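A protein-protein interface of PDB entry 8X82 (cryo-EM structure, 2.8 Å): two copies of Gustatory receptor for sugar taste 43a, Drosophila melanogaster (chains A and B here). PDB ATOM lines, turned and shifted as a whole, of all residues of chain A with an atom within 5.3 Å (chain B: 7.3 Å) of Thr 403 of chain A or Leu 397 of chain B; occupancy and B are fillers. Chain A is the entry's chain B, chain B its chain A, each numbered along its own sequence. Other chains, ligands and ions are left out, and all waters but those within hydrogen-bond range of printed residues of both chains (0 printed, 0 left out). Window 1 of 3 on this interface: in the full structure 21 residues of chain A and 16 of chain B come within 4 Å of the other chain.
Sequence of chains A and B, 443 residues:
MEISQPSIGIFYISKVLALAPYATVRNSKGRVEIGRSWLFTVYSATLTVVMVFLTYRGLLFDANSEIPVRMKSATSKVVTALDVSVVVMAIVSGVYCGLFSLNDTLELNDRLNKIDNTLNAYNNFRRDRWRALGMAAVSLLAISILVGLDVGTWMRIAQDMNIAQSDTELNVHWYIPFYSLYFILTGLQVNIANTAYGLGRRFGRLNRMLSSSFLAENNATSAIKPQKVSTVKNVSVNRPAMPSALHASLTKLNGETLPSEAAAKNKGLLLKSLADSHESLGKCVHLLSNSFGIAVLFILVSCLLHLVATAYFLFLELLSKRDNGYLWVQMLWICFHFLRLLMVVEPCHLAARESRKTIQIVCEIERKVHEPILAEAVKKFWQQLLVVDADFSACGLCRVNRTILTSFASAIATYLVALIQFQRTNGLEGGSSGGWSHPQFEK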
ATOM      1  N   ASN A 401      -6.869   7.571  18.673  1.00  0.00           N
ATOM      2  CA  ASN A 401      -7.475   7.570  17.350  1.00  0.00           C
ATOM      3  C   ASN A 401      -7.381   8.989  16.803  1.00  0.00           C
ATOM      4  O   ASN A 401      -6.703   9.849  17.373  1.00  0.00           O
ATOM      5  CB  ASN A 401      -8.916   7.047  17.402  1.00  0.00           C
ATOM      6  CG  ASN A 401      -9.669   7.528  18.624  1.00  0.00           C
ATOM      7  OD1 ASN A 401      -9.591   8.697  18.994  1.00  0.00           O
ATOM      8  ND2 ASN A 401     -10.407   6.626  19.256  1.00  0.00           N
ATOM      9  N   ARG A 402      -8.073   9.245  15.692  1.00  0.00           N
ATOM     10  CA  ARG A 402      -7.993  10.558  15.065  1.00  0.00           C
ATOM     11  C   ARG A 402      -8.744  11.626  15.849  1.00  0.00           C
ATOM     12  O   ARG A 402      -8.578  12.815  15.564  1.00  0.00           O
ATOM     13  CB  ARG A 402      -8.512  10.482  13.631  1.00  0.00           C
ATOM     14  CG  ARG A 402      -7.433  10.138  12.620  1.00  0.00           C
ATOM     15  CD  ARG A 402      -8.000  10.041  11.223  1.00  0.00           C
ATOM     16  NE  ARG A 402      -7.152   9.256  10.337  1.00  0.00           N
ATOM     17  CZ  ARG A 402      -7.461   8.953   9.085  1.00  0.00           C
ATOM     18  NH1 ARG A 402      -8.600   9.347   8.540  1.00  0.00           N
ATOM     19  NH2 ARG A 402      -6.606   8.235   8.361  1.00  0.00           N
ATOM     20  N   THR A 403      -9.567  11.232  16.823  1.00  0.00           N
ATOM     21  CA  THR A 403     -10.174  12.202  17.729  1.00  0.00           C
ATOM     22  C   THR A 403      -9.121  12.913  18.573  1.00  0.00           C
ATOM     23  O   THR A 403      -9.299  14.090  18.915  1.00  0.00           O
ATOM     24  CB  THR A 403     -11.206  11.496  18.617  1.00  0.00           C
ATOM     25  OG1 THR A 403     -12.398  11.253  17.859  1.00  0.00           O
ATOM     26  CG2 THR A 403     -11.563  12.333  19.839  1.00  0.00           C
ATOM     27  N   ILE A 404      -8.015  12.231  18.883  1.00  0.00           N
ATOM     28  CA  ILE A 404      -6.904  12.859  19.589  1.00  0.00           C
ATOM     29  C   ILE A 404      -6.377  14.055  18.810  1.00  0.00           C
ATOM     30  O   ILE A 404      -5.945  15.049  19.402  1.00  0.00           O
ATOM     31  CB  ILE A 404      -5.800  11.818  19.860  1.00  0.00           C
ATOM     32  CG1 ILE A 404      -6.224  10.873  20.984  1.00  0.00           C
ATOM     33  CG2 ILE A 404      -4.472  12.488  20.181  1.00  0.00           C
ATOM     34  CD1 ILE A 404      -5.070  10.189  21.678  1.00  0.00           C
ATOM     35  N   LEU A 405      -6.414  13.991  17.478  1.00  0.00           N
ATOM     36  CA  LEU A 405      -5.980  15.126  16.672  1.00  0.00           C
ATOM     37  C   LEU A 405      -6.858  16.348  16.918  1.00  0.00           C
ATOM     38  O   LEU A 405      -6.353  17.470  17.031  1.00  0.00           O
ATOM     39  CB  LEU A 405      -5.989  14.751  15.192  1.00  0.00           C
ATOM     40  CG  LEU A 405      -5.026  13.650  14.752  1.00  0.00           C
ATOM     41  CD1 LEU A 405      -5.144  13.420  13.257  1.00  0.00           C
ATOM     42  CD2 LEU A 405      -3.600  14.003  15.134  1.00  0.00           C
ATOM     43  N   THR A 406      -8.176  16.149  16.999  1.00  0.00           N
ATOM     44  CA  THR A 406      -9.076  17.264  17.284  1.00  0.00           C
ATOM     45  C   THR A 406      -8.833  17.826  18.678  1.00  0.00           C
ATOM     46  O   THR A 406      -8.791  19.049  18.867  1.00  0.00           O
ATOM     47  CB  THR A 406     -10.530  16.817  17.133  1.00  0.00           C
ATOM     48  OG1 THR A 406     -10.739  16.303  15.813  1.00  0.00           O
ATOM     49  CG2 THR A 406     -11.474  17.984  17.370  1.00  0.00           C
ATOM     50  N   SER A 407      -8.668  16.947  19.669  1.00  0.00           N
ATOM     51  CA  SER A 407      -8.381  17.407  21.025  1.00  0.00           C
ATOM     52  C   SER A 407      -7.049  18.142  21.083  1.00  0.00           C
ATOM     53  O   SER A 407      -6.921  19.164  21.766  1.00  0.00           O
ATOM     54  CB  SER A 407      -8.386  16.226  21.993  1.00  0.00           C
ATOM     55  OG  SER A 407      -9.639  15.564  21.983  1.00  0.00           O
ATOM     56  N   PHE A 408      -6.043  17.630  20.369  1.00  0.00           N
ATOM     57  CA  PHE A 408      -4.745  18.292  20.313  1.00  0.00           C
ATOM     58  C   PHE A 408      -4.854  19.666  19.668  1.00  0.00           C
ATOM     59  O   PHE A 408      -4.244  20.628  20.142  1.00  0.00           O
ATOM     60  CB  PHE A 408      -3.752  17.420  19.549  1.00  0.00           C
ATOM     61  CG  PHE A 408      -2.916  16.538  20.427  1.00  0.00           C
ATOM     62  CD1 PHE A 408      -3.509  15.712  21.366  1.00  0.00           C
ATOM     63  CD2 PHE A 408      -1.539  16.517  20.300  1.00  0.00           C
ATOM     64  CE1 PHE A 408      -2.743  14.896  22.173  1.00  0.00           C
ATOM     65  CE2 PHE A 408      -0.770  15.700  21.101  1.00  0.00           C
ATOM     66  CZ  PHE A 408      -1.371  14.890  22.038  1.00  0.00           C
ATOM     67  N   ILE B 294     -13.035  15.064   4.142  1.00  0.00           N
ATOM     68  CA  ILE B 294     -12.079  16.152   4.314  1.00  0.00           C
ATOM     69  C   ILE B 294     -12.697  17.475   3.876  1.00  0.00           C
ATOM     70  O   ILE B 294     -12.393  18.533   4.439  1.00  0.00           O
ATOM     71  CB  ILE B 294     -10.766  15.841   3.567  1.00  0.00           C
ATOM     72  CG1 ILE B 294      -9.657  16.793   4.015  1.00  0.00           C
ATOM     73  CG2 ILE B 294     -10.952  15.903   2.064  1.00  0.00           C
ATOM     74  CD1 ILE B 294      -8.776  16.233   5.108  1.00  0.00           C
ATOM     75  N   LEU B 297     -14.813  18.442   6.797  1.00  0.00           N
ATOM     76  CA  LEU B 297     -13.941  18.862   7.891  1.00  0.00           C
ATOM     77  C   LEU B 297     -13.407  20.269   7.663  1.00  0.00           C
ATOM     78  O   LEU B 297     -13.374  21.087   8.590  1.00  0.00           O
ATOM     79  CB  LEU B 297     -12.790  17.871   8.052  1.00  0.00           C
ATOM     80  CG  LEU B 297     -11.758  18.203   9.129  1.00  0.00           C
ATOM     81  CD1 LEU B 297     -12.308  17.895  10.510  1.00  0.00           C
ATOM     82  CD2 LEU B 297     -10.467  17.446   8.880  1.00  0.00           C
ATOM     83  N   SER B 393     -19.019  10.773   9.732  1.00  0.00           N
ATOM     84  CA  SER B 393     -17.686  11.023  10.260  1.00  0.00           C
ATOM     85  C   SER B 393     -16.868  11.813   9.248  1.00  0.00           C
ATOM     86  O   SER B 393     -16.805  11.445   8.071  1.00  0.00           O
ATOM     87  CB  SER B 393     -16.982   9.709  10.599  1.00  0.00           C
ATOM     88  OG  SER B 393     -15.723   9.949  11.199  1.00  0.00           O
ATOM     89  N   ALA B 394     -16.242  12.896   9.712  1.00  0.00           N
ATOM     90  CA  ALA B 394     -15.361  13.706   8.872  1.00  0.00           C
ATOM     91  C   ALA B 394     -13.931  13.208   9.056  1.00  0.00           C
ATOM     92  O   ALA B 394     -13.137  13.753   9.825  1.00  0.00           O
ATOM     93  CB  ALA B 394     -15.498  15.184   9.217  1.00  0.00           C
ATOM     94  N   CYS B 395     -13.608  12.137   8.329  1.00  0.00           N
ATOM     95  CA  CYS B 395     -12.309  11.470   8.372  1.00  0.00           C
ATOM     96  C   CYS B 395     -11.950  10.961   9.760  1.00  0.00           C
ATOM     97  O   CYS B 395     -10.769  10.787  10.067  1.00  0.00           O
ATOM     98  CB  CYS B 395     -11.189  12.381   7.855  1.00  0.00           C
ATOM     99  SG  CYS B 395     -11.557  13.228   6.311  1.00  0.00           S
ATOM    100  N   GLY B 396     -12.941  10.716  10.613  1.00  0.00           N
ATOM    101  CA  GLY B 396     -12.680  10.262  11.961  1.00  0.00           C
ATOM    102  C   GLY B 396     -12.268  11.342  12.933  1.00  0.00           C
ATOM    103  O   GLY B 396     -12.113  11.048  14.123  1.00  0.00           O
ATOM    104  N   LEU B 397     -12.085  12.578  12.467  1.00  0.00           N
ATOM    105  CA  LEU B 397     -11.727  13.671  13.362  1.00  0.00           C
ATOM    106  C   LEU B 397     -12.861  13.994  14.325  1.00  0.00           C
ATOM    107  O   LEU B 397     -12.623  14.242  15.512  1.00  0.00           O
ATOM    108  CB  LEU B 397     -11.349  14.913  12.553  1.00  0.00           C
ATOM    109  CG  LEU B 397      -9.906  15.067  12.064  1.00  0.00           C
ATOM    110  CD1 LEU B 397      -8.959  15.178  13.239  1.00  0.00           C
ATOM    111  CD2 LEU B 397      -9.492  13.929  11.144  1.00  0.00           C
ATOM    112  N   CYS B 398     -14.096  13.995  13.830  1.00  0.00           N
ATOM    113  CA  CYS B 398     -15.254  14.297  14.655  1.00  0.00           C
ATOM    114  C   CYS B 398     -16.486  13.686  14.008  1.00  0.00           C
ATOM    115  O   CYS B 398     -16.498  13.383  12.813  1.00  0.00           O
ATOM    116  CB  CYS B 398     -15.434  15.807  14.839  1.00  0.00           C
ATOM    117  SG  CYS B 398     -15.827  16.694  13.316  1.00  0.00           S
ATOM    118  N   ARG B 399     -17.525  13.509  14.819  1.00  0.00           N
ATOM    119  CA  ARG B 399     -18.808  13.021  14.339  1.00  0.00           C
ATOM    120  C   ARG B 399     -19.720  14.211  14.072  1.00  0.00           C
ATOM    121  O   ARG B 399     -19.952  15.033  14.963  1.00  0.00           O
ATOM    122  CB  ARG B 399     -19.439  12.073  15.358  1.00  0.00           C
ATOM    123  CG  ARG B 399     -19.401  10.613  14.939  1.00  0.00           C
ATOM    124  CD  ARG B 399     -19.787   9.694  16.086  1.00  0.00           C
ATOM    125  NE  ARG B 399     -19.216  10.131  17.354  1.00  0.00           N
ATOM    126  CZ  ARG B 399     -19.823  10.019  18.527  1.00  0.00           C
ATOM    127  NH1 ARG B 399     -21.030   9.491  18.634  1.00  0.00           N
ATOM    128  NH2 ARG B 399     -19.200  10.447  19.623  1.00  0.00           N
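Thr 403 of chain A touches just these residues of chain B: Gly 396 (3.7 Å) and Leu 397 (3.8 Å). Of the printed residues of chain A, Gly 396 of chain B touches Arg 402 (3.7 Å) and Thr 403 (3.7 Å). Printed residues of chain A within 4 Å of Cys 395 of chain B: Arg 402 (3.0 Å). Printed residues of chain B within 4 Å of Leu 405 of chain A: Leu 397. Printed residues of chain B within 4 Å of Arg 402 of chain A: Cys 395, Gly 396 and Leu 397. Of the printed residues of chain B, Thr 406 of chain A touches Leu 397. Asn 401 of chain A touches none of the printed residues of chain B. Ala 394 of chain B touches none of the printed residues of chain A. The nearest residue of chain B that does not touch Thr 403 of chain A is Cys 398 of chain B (5.2 Å). The nearest printed residue of chain A that does not touch Leu 397 of chain B is Ile 404 of chain A (6.1 Å). The nearest printed residue of chain B that does not touch Arg 402 of chain A is Cys 398 of chain B (5.9 Å).
The backbone carbonyl oxygen (O) of Leu 397 of chain B is in hydrogen-bond range of the side-chain hydroxyl (OG1) of Thr 406 of chain A (2.8 Å). O of Cys 395 of chain B sits at hydrogen-bond distance from NH1 of Arg 402 of chain A.
SG of Cys 395 of chain B sits at hydrogen-bond distance from N of Ile 294 of chain B. The side-chain hydroxyl (OG) of Ser 393 of chain B lies within hydrogen-bond range of the backbone NH (N) of Gly 396 of chain B, 2.9 Å away. N of Thr 403 of chain A lies close to OD1 of Asn 401 of chain A, at 3.3 Å. The backbone carbonyl oxygen of Thr 403 of chain A is in hydrogen-bond range of the side-chain hydroxyl of Ser 407 of chain A, 3.4 Å away.
No position is printed for both chains.
Among the printed residues, merely in contact across the chains: Arg 402 of chain A with Gly 396 of chain B (3.7 Å), Arg 402 of chain A with Leu 397 of chain B (3.3 Å), Thr 403 of chain A with Gly 396 of chain B (3.7 Å), Thr 403 of chain A with Leu 397 of chain B (3.8 Å) and Leu 405 of chain A with Leu 397 of chain B (3.6 Å).
Of the 8 printed residues of chain A, 4 touch a printed residue of chain B. Printed residues of chain A that touch a printed residue of chain B: Arg 402, Thr 403, Leu 405 and Thr 406. Hydrophobic or aromatic side chains of chain A that line the printed part of chain B: Leu 405. Of the 9 printed residues of chain B, 3 touch a printed residue of chain A. Among the printed residues, no Asp or Glu carboxylate lies within 4 Å of a Lys or Arg side-chain nitrogen of the other chain.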
